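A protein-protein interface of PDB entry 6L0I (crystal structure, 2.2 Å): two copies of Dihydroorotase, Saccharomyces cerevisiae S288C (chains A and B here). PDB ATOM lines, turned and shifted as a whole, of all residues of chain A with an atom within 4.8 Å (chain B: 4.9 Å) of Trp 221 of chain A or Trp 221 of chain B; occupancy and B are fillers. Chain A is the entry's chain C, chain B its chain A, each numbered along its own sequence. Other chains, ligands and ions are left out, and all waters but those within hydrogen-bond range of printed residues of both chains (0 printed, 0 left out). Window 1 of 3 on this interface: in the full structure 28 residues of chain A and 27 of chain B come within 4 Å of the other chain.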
ATOM      1  N   THR A 217      14.683  -0.417 -12.063  1.00  0.00           N
ATOM      2  CA  THR A 217      14.391   0.828 -11.368  1.00  0.00           C
ATOM      3  C   THR A 217      12.893   1.103 -11.485  1.00  0.00           C
ATOM      4  O   THR A 217      12.138   0.327 -12.091  1.00  0.00           O
ATOM      5  CB  THR A 217      15.195   1.996 -11.941  1.00  0.00           C
ATOM      6  OG1 THR A 217      14.759   2.237 -13.275  1.00  0.00           O
ATOM      7  CG2 THR A 217      16.691   1.678 -11.964  1.00  0.00           C
ATOM      8  N   ILE A 218      12.463   2.222 -10.891  1.00  0.00           N
ATOM      9  CA  ILE A 218      11.040   2.539 -10.854  1.00  0.00           C
ATOM     10  C   ILE A 218      10.464   2.555 -12.259  1.00  0.00           C
ATOM     11  O   ILE A 218       9.325   2.114 -12.475  1.00  0.00           O
ATOM     12  CB  ILE A 218      10.788   3.871 -10.110  1.00  0.00           C
ATOM     13  CG1 ILE A 218       9.290   4.206 -10.106  1.00  0.00           C
ATOM     14  CG2 ILE A 218      11.575   4.999 -10.729  1.00  0.00           C
ATOM     15  CD1 ILE A 218       8.845   5.039  -8.921  1.00  0.00           C
ATOM     16  N   ASP A 219      11.256   2.988 -13.241  1.00  0.00           N
ATOM     17  CA  ASP A 219      10.750   3.077 -14.602  1.00  0.00           C
ATOM     18  C   ASP A 219      10.381   1.719 -15.186  1.00  0.00           C
ATOM     19  O   ASP A 219       9.555   1.660 -16.097  1.00  0.00           O
ATOM     20  CB  ASP A 219      11.773   3.752 -15.498  1.00  0.00           C
ATOM     21  CG  ASP A 219      11.580   5.250 -15.564  1.00  0.00           C
ATOM     22  OD1 ASP A 219      11.182   5.847 -14.540  1.00  0.00           O
ATOM     23  OD2 ASP A 219      11.834   5.828 -16.632  1.00  0.00           O
ATOM     24  N   ASP A 220      10.982   0.626 -14.712  1.00  0.00           N
ATOM     25  CA  ASP A 220      10.669  -0.674 -15.294  1.00  0.00           C
ATOM     26  C   ASP A 220       9.330  -1.223 -14.838  1.00  0.00           C
ATOM     27  O   ASP A 220       8.754  -2.062 -15.535  1.00  0.00           O
ATOM     28  CB  ASP A 220      11.758  -1.693 -14.972  1.00  0.00           C
ATOM     29  CG  ASP A 220      13.090  -1.330 -15.575  1.00  0.00           C
ATOM     30  OD1 ASP A 220      13.182  -1.273 -16.817  1.00  0.00           O
ATOM     31  OD2 ASP A 220      14.054  -1.101 -14.807  1.00  0.00           O
ATOM     32  N   TRP A 221       8.821  -0.798 -13.678  1.00  0.00           N
ATOM     33  CA  TRP A 221       7.536  -1.295 -13.225  1.00  0.00           C
ATOM     34  C   TRP A 221       6.437  -0.240 -13.289  1.00  0.00           C
ATOM     35  O   TRP A 221       5.262  -0.583 -13.092  1.00  0.00           O
ATOM     36  CB  TRP A 221       7.650  -1.885 -11.799  1.00  0.00           C
ATOM     37  CG  TRP A 221       8.120  -0.954 -10.698  1.00  0.00           C
ATOM     38  CD1 TRP A 221       9.420  -0.761 -10.254  1.00  0.00           C
ATOM     39  CD2 TRP A 221       7.293  -0.110  -9.882  1.00  0.00           C
ATOM     40  NE1 TRP A 221       9.435   0.155  -9.233  1.00  0.00           N
ATOM     41  CE2 TRP A 221       8.150   0.574  -8.982  1.00  0.00           C
ATOM     42  CE3 TRP A 221       5.911   0.137  -9.827  1.00  0.00           C
ATOM     43  CZ2 TRP A 221       7.667   1.497  -8.050  1.00  0.00           C
ATOM     44  CZ3 TRP A 221       5.433   1.042  -8.893  1.00  0.00           C
ATOM     45  CH2 TRP A 221       6.306   1.711  -8.013  1.00  0.00           C
ATOM     46  N   ALA A 222       6.782   1.023 -13.545  1.00  0.00           N
ATOM     47  CA  ALA A 222       5.790   2.064 -13.791  1.00  0.00           C
ATOM     48  C   ALA A 222       5.073   1.716 -15.088  1.00  0.00           C
ATOM     49  O   ALA A 222       5.581   1.976 -16.183  1.00  0.00           O
ATOM     50  CB  ALA A 222       6.457   3.431 -13.878  1.00  0.00           C
ATOM     51  N   GLY A 223       3.922   1.068 -14.980  1.00  0.00           N
ATOM     52  CA  GLY A 223       3.239   0.587 -16.157  1.00  0.00           C
ATOM     53  C   GLY A 223       3.472  -0.865 -16.526  1.00  0.00           C
ATOM     54  O   GLY A 223       2.996  -1.292 -17.585  1.00  0.00           O
ATOM     55  N   ASN A 224       4.168  -1.644 -15.693  1.00  0.00           N
ATOM     56  CA  ASN A 224       4.450  -3.051 -15.993  1.00  0.00           C
ATOM     57  C   ASN A 224       4.324  -3.888 -14.737  1.00  0.00           C
ATOM     58  O   ASN A 224       5.319  -4.141 -14.040  1.00  0.00           O
ATOM     59  CB  ASN A 224       5.840  -3.223 -16.597  1.00  0.00           C
ATOM     60  CG  ASN A 224       5.997  -2.480 -17.892  1.00  0.00           C
ATOM     61  OD1 ASN A 224       5.211  -2.666 -18.818  1.00  0.00           O
ATOM     62  ND2 ASN A 224       7.023  -1.637 -17.976  1.00  0.00           N
ATOM     63  N   PRO A 225       3.110  -4.345 -14.417  1.00  0.00           N
ATOM     64  CA  PRO A 225       2.923  -5.155 -13.206  1.00  0.00           C
ATOM     65  C   PRO A 225       3.826  -6.369 -13.125  1.00  0.00           C
ATOM     66  O   PRO A 225       4.161  -6.792 -12.013  1.00  0.00           O
ATOM     67  CB  PRO A 225       1.440  -5.547 -13.283  1.00  0.00           C
ATOM     68  CG  PRO A 225       0.799  -4.379 -14.020  1.00  0.00           C
ATOM     69  CD  PRO A 225       1.821  -3.953 -15.029  1.00  0.00           C
ATOM     70  N   ASN A 227       6.840  -6.476 -13.453  1.00  0.00           N
ATOM     71  CA  ASN A 227       8.045  -6.066 -12.750  1.00  0.00           C
ATOM     72  C   ASN A 227       7.762  -5.477 -11.377  1.00  0.00           C
ATOM     73  O   ASN A 227       8.688  -4.970 -10.729  1.00  0.00           O
ATOM     74  CB  ASN A 227       8.825  -5.068 -13.593  1.00  0.00           C
ATOM     75  CG  ASN A 227       9.474  -5.728 -14.799  1.00  0.00           C
ATOM     76  OD1 ASN A 227       9.898  -6.883 -14.724  1.00  0.00           O
ATOM     77  ND2 ASN A 227       9.553  -4.998 -15.917  1.00  0.00           N
ATOM     78  N   PHE A 228       6.515  -5.544 -10.914  1.00  0.00           N
ATOM     79  CA  PHE A 228       6.120  -4.974  -9.629  1.00  0.00           C
ATOM     80  C   PHE A 228       6.331  -6.021  -8.542  1.00  0.00           C
ATOM     81  O   PHE A 228       5.779  -7.123  -8.622  1.00  0.00           O
ATOM     82  CB  PHE A 228       4.663  -4.516  -9.662  1.00  0.00           C
ATOM     83  CG  PHE A 228       4.108  -4.149  -8.319  1.00  0.00           C
ATOM     84  CD1 PHE A 228       4.655  -3.123  -7.579  1.00  0.00           C
ATOM     85  CD2 PHE A 228       3.027  -4.823  -7.807  1.00  0.00           C
ATOM     86  CE1 PHE A 228       4.127  -2.790  -6.322  1.00  0.00           C
ATOM     87  CE2 PHE A 228       2.494  -4.502  -6.567  1.00  0.00           C
ATOM     88  CZ  PHE A 228       3.031  -3.493  -5.822  1.00  0.00           C
ATOM     89  N   VAL A 232       9.613  -2.333  -3.600  1.00  0.00           N
ATOM     90  CA  VAL A 232       9.616  -1.917  -4.994  1.00  0.00           C
ATOM     91  C   VAL A 232      11.017  -1.458  -5.431  1.00  0.00           C
ATOM     92  O   VAL A 232      11.788  -0.892  -4.632  1.00  0.00           O
ATOM     93  CB  VAL A 232       8.544  -0.819  -5.088  1.00  0.00           C
ATOM     94  CG1 VAL A 232       9.084   0.591  -4.726  1.00  0.00           C
ATOM     95  CG2 VAL A 232       7.733  -0.947  -6.337  1.00  0.00           C
ATOM     96  N   ALA A 233      11.367  -1.740  -6.689  1.00  0.00           N
ATOM     97  CA  ALA A 233      12.605  -1.204  -7.228  1.00  0.00           C
ATOM     98  C   ALA A 233      12.550   0.315  -7.259  1.00  0.00           C
ATOM     99  O   ALA A 233      11.530   0.924  -7.628  1.00  0.00           O
ATOM    100  CB  ALA A 233      12.896  -1.736  -8.632  1.00  0.00           C
ATOM    101  N   THR B 217      -1.267   9.257  -4.312  1.00  0.00           N
ATOM    102  CA  THR B 217       0.188   9.216  -4.171  1.00  0.00           C
ATOM    103  C   THR B 217       0.690   7.971  -4.883  1.00  0.00           C
ATOM    104  O   THR B 217      -0.093   7.163  -5.385  1.00  0.00           O
ATOM    105  CB  THR B 217       0.654   9.164  -2.712  1.00  0.00           C
ATOM    106  OG1 THR B 217       0.206   7.940  -2.144  1.00  0.00           O
ATOM    107  CG2 THR B 217       0.125  10.353  -1.876  1.00  0.00           C
ATOM    108  N   ILE B 218       2.015   7.803  -4.914  1.00  0.00           N
ATOM    109  CA  ILE B 218       2.609   6.602  -5.515  1.00  0.00           C
ATOM    110  C   ILE B 218       2.054   5.317  -4.892  1.00  0.00           C
ATOM    111  O   ILE B 218       1.907   4.292  -5.576  1.00  0.00           O
ATOM    112  CB  ILE B 218       4.145   6.662  -5.406  1.00  0.00           C
ATOM    113  CG1 ILE B 218       4.779   5.474  -6.131  1.00  0.00           C
ATOM    114  CG2 ILE B 218       4.592   6.722  -3.940  1.00  0.00           C
ATOM    115  CD1 ILE B 218       6.260   5.602  -6.315  1.00  0.00           C
ATOM    116  N   ASP B 219       1.721   5.350  -3.598  1.00  0.00           N
ATOM    117  CA  ASP B 219       1.160   4.173  -2.938  1.00  0.00           C
ATOM    118  C   ASP B 219      -0.147   3.728  -3.578  1.00  0.00           C
ATOM    119  O   ASP B 219      -0.504   2.548  -3.509  1.00  0.00           O
ATOM    120  CB  ASP B 219       0.944   4.472  -1.451  1.00  0.00           C
ATOM    121  CG  ASP B 219       2.181   4.210  -0.636  1.00  0.00           C
ATOM    122  OD1 ASP B 219       2.089   3.785   0.529  1.00  0.00           O
ATOM    123  OD2 ASP B 219       3.271   4.418  -1.186  1.00  0.00           O
ATOM    124  N   ASP B 220      -0.869   4.639  -4.217  1.00  0.00           N
ATOM    125  CA  ASP B 220      -2.167   4.274  -4.755  1.00  0.00           C
ATOM    126  C   ASP B 220      -2.104   3.645  -6.140  1.00  0.00           C
ATOM    127  O   ASP B 220      -3.040   2.926  -6.506  1.00  0.00           O
ATOM    128  CB  ASP B 220      -3.083   5.501  -4.774  1.00  0.00           C
ATOM    129  CG  ASP B 220      -3.310   6.074  -3.385  1.00  0.00           C
ATOM    130  OD1 ASP B 220      -3.720   5.302  -2.502  1.00  0.00           O
ATOM    131  OD2 ASP B 220      -3.067   7.282  -3.158  1.00  0.00           O
ATOM    132  N   TRP B 221      -1.047   3.878  -6.930  1.00  0.00           N
ATOM    133  CA  TRP B 221      -0.980   3.255  -8.248  1.00  0.00           C
ATOM    134  C   TRP B 221       0.062   2.145  -8.356  1.00  0.00           C
ATOM    135  O   TRP B 221       0.083   1.445  -9.376  1.00  0.00           O
ATOM    136  CB  TRP B 221      -0.740   4.307  -9.355  1.00  0.00           C
ATOM    137  CG  TRP B 221       0.526   5.096  -9.229  1.00  0.00           C
ATOM    138  CD1 TRP B 221       0.671   6.329  -8.655  1.00  0.00           C
ATOM    139  CD2 TRP B 221       1.819   4.715  -9.694  1.00  0.00           C
ATOM    140  NE1 TRP B 221       1.970   6.733  -8.726  1.00  0.00           N
ATOM    141  CE2 TRP B 221       2.704   5.765  -9.364  1.00  0.00           C
ATOM    142  CE3 TRP B 221       2.316   3.593 -10.368  1.00  0.00           C
ATOM    143  CZ2 TRP B 221       4.063   5.725  -9.665  1.00  0.00           C
ATOM    144  CZ3 TRP B 221       3.672   3.546 -10.661  1.00  0.00           C
ATOM    145  CH2 TRP B 221       4.530   4.614 -10.308  1.00  0.00           C
ATOM    146  N   ALA B 222       0.888   1.927  -7.327  1.00  0.00           N
ATOM    147  CA  ALA B 222       1.959   0.933  -7.421  1.00  0.00           C
ATOM    148  C   ALA B 222       1.419  -0.443  -7.819  1.00  0.00           C
ATOM    149  O   ALA B 222       1.893  -1.060  -8.781  1.00  0.00           O
ATOM    150  CB  ALA B 222       2.718   0.866  -6.095  1.00  0.00           C
ATOM    151  N   GLY B 223       0.414  -0.935  -7.111  1.00  0.00           N
ATOM    152  CA  GLY B 223      -0.189  -2.185  -7.525  1.00  0.00           C
ATOM    153  C   GLY B 223      -1.585  -2.053  -8.094  1.00  0.00           C
ATOM    154  O   GLY B 223      -2.306  -3.055  -8.180  1.00  0.00           O
ATOM    155  N   ASN B 224      -1.980  -0.838  -8.497  1.00  0.00           N
ATOM    156  CA  ASN B 224      -3.330  -0.559  -8.997  1.00  0.00           C
ATOM    157  C   ASN B 224      -3.237   0.197 -10.315  1.00  0.00           C
ATOM    158  O   ASN B 224      -3.163   1.434 -10.330  1.00  0.00           O
ATOM    159  CB  ASN B 224      -4.156   0.246  -7.995  1.00  0.00           C
ATOM    160  CG  ASN B 224      -4.414  -0.499  -6.693  1.00  0.00           C
ATOM    161  OD1 ASN B 224      -4.950  -1.613  -6.678  1.00  0.00           O
ATOM    162  ND2 ASN B 224      -4.037   0.128  -5.583  1.00  0.00           N
ATOM    163  N   PRO B 225      -3.240  -0.519 -11.445  1.00  0.00           N
ATOM    164  CA  PRO B 225      -3.165   0.142 -12.761  1.00  0.00           C
ATOM    165  C   PRO B 225      -4.278   1.155 -13.054  1.00  0.00           C
ATOM    166  O   PRO B 225      -4.057   2.081 -13.843  1.00  0.00           O
ATOM    167  CB  PRO B 225      -3.230  -1.043 -13.729  1.00  0.00           C
ATOM    168  CG  PRO B 225      -2.646  -2.182 -12.954  1.00  0.00           C
ATOM    169  CD  PRO B 225      -3.056  -1.978 -11.539  1.00  0.00           C
ATOM    170  N   ASN B 227      -5.151   3.429 -11.256  1.00  0.00           N
ATOM    171  CA  ASN B 227      -4.651   4.703 -10.759  1.00  0.00           C
ATOM    172  C   ASN B 227      -3.358   5.138 -11.447  1.00  0.00           C
ATOM    173  O   ASN B 227      -2.812   6.187 -11.104  1.00  0.00           O
ATOM    174  CB  ASN B 227      -4.462   4.631  -9.236  1.00  0.00           C
ATOM    175  CG  ASN B 227      -5.799   4.612  -8.472  1.00  0.00           C
ATOM    176  OD1 ASN B 227      -6.836   5.055  -8.977  1.00  0.00           O
ATOM    177  ND2 ASN B 227      -5.773   4.085  -7.261  1.00  0.00           N
ATOM    178  N   PHE B 228      -2.866   4.367 -12.413  1.00  0.00           N
ATOM    179  CA  PHE B 228      -1.642   4.711 -13.126  1.00  0.00           C
ATOM    180  C   PHE B 228      -1.972   5.754 -14.172  1.00  0.00           C
ATOM    181  O   PHE B 228      -2.894   5.568 -14.970  1.00  0.00           O
ATOM    182  CB  PHE B 228      -1.025   3.471 -13.796  1.00  0.00           C
ATOM    183  CG  PHE B 228       0.217   3.770 -14.622  1.00  0.00           C
ATOM    184  CD1 PHE B 228       1.338   4.375 -14.047  1.00  0.00           C
ATOM    185  CD2 PHE B 228       0.267   3.437 -15.976  1.00  0.00           C
ATOM    186  CE1 PHE B 228       2.487   4.649 -14.807  1.00  0.00           C
ATOM    187  CE2 PHE B 228       1.421   3.709 -16.741  1.00  0.00           C
ATOM    188  CZ  PHE B 228       2.529   4.323 -16.150  1.00  0.00           C
ATOM    189  N   VAL B 232       3.117  10.503 -13.214  1.00  0.00           N
ATOM    190  CA  VAL B 232       2.673   9.653 -12.121  1.00  0.00           C
ATOM    191  C   VAL B 232       2.423  10.496 -10.875  1.00  0.00           C
ATOM    192  O   VAL B 232       3.050  11.543 -10.668  1.00  0.00           O
ATOM    193  CB  VAL B 232       3.704   8.543 -11.847  1.00  0.00           C
ATOM    194  CG1 VAL B 232       4.000   7.765 -13.130  1.00  0.00           C
ATOM    195  CG2 VAL B 232       4.990   9.120 -11.203  1.00  0.00           C
ATOM    196  N   ALA B 233       1.498  10.033 -10.033  1.00  0.00           N
ATOM    197  CA  ALA B 233       1.351  10.609  -8.697  1.00  0.00           C
ATOM    198  C   ALA B 233       2.571  10.307  -7.827  1.00  0.00           C
ATOM    199  O   ALA B 233       3.059   9.172  -7.779  1.00  0.00           O
ATOM    200  CB  ALA B 233       0.087  10.074  -8.024  1.00  0.00           C
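The backbone NH (N) of Ile 218 of chain B sits at hydrogen-bond distance from the backbone carbonyl oxygen (O) of Ala 233 of chain B (3.3 Å). NE1 of Trp 221 of chain B sits at hydrogen-bond distance from O of Ala 233 of chain B. The indole nitrogen (NE1) of Trp 221 of chain A sits at hydrogen-bond distance from the backbone carbonyl oxygen (O) of Ala 233 of chain A, 2.7 Å away.
Among the printed residues, pairs that only touch across the chains: Ile 218 of chain A with Ile 218 of chain B, Trp 221 of chain A with Trp 221 of chain B, Trp 221 of chain A with Ala 222 of chain B, Ala 222 of chain A with Phe 228 of chain B, Gly 223 of chain A with Phe 228 of chain B, Phe 228 of chain A with Ala 222 of chain B and Phe 228 of chain A with Gly 223 of chain B.
Trp 221 of chain A touches just these residues of chain B: Trp 221 and Ala 222. Trp 221 of chain B touches just one residue of chain A: Trp 221. Of the printed residues of chain A, Ile 218 of chain B touches Ile 218 (3.7 Å). Printed residues of chain B within 4 Å of Ala 222 of chain A: Phe 228 (3.8 Å). Of the printed residues of chain B, Phe 228 of chain A touches Ala 222 and Gly 223. Of the printed residues of chain A, Phe 228 of chain B touches Ala 222 and Gly 223. Printed residues of chain A within 4 Å of Gly 223 of chain B: Phe 228. Thr 217 of chain A touches none of the printed residues of chain B. The nearest residue of chain B that does not touch Trp 221 of chain A is Ile 218 of chain B (4.2 Å). The nearest residue of chain A that does not touch Trp 221 of chain B is Ala 222 of chain A (4.1 Å). The nearest printed residue of chain A that does not touch Ala 222 of chain B is Val 232 of chain A (5.3 Å).
Of the 13 printed residues of chain A, 5 touch a printed residue of chain B. Hydrophobic or aromatic side chains of chain B within 4 Å of the printed part of chain A: Ile 218, Trp 221, Ala 222 and Phe 228. Among the printed residues, no Asp or Glu carboxylate lies within 4 Å of a Lys or Arg side-chain nitrogen of the other chain.
Ile 218 of chain A touches its own counterpart, Ile 218 of chain B. Trp 221 of chain A touches its own counterpart, Trp 221 of chain B. Ala 222 of chain A touches Phe 228 of chain B, and with the chains exchanged Phe 228 of chain A touches Ala 222 of chain B. Gly 223 of chain A touches Phe 228 of chain B, and with the chains exchanged Phe 228 of chain A touches Gly 223 of chain B.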
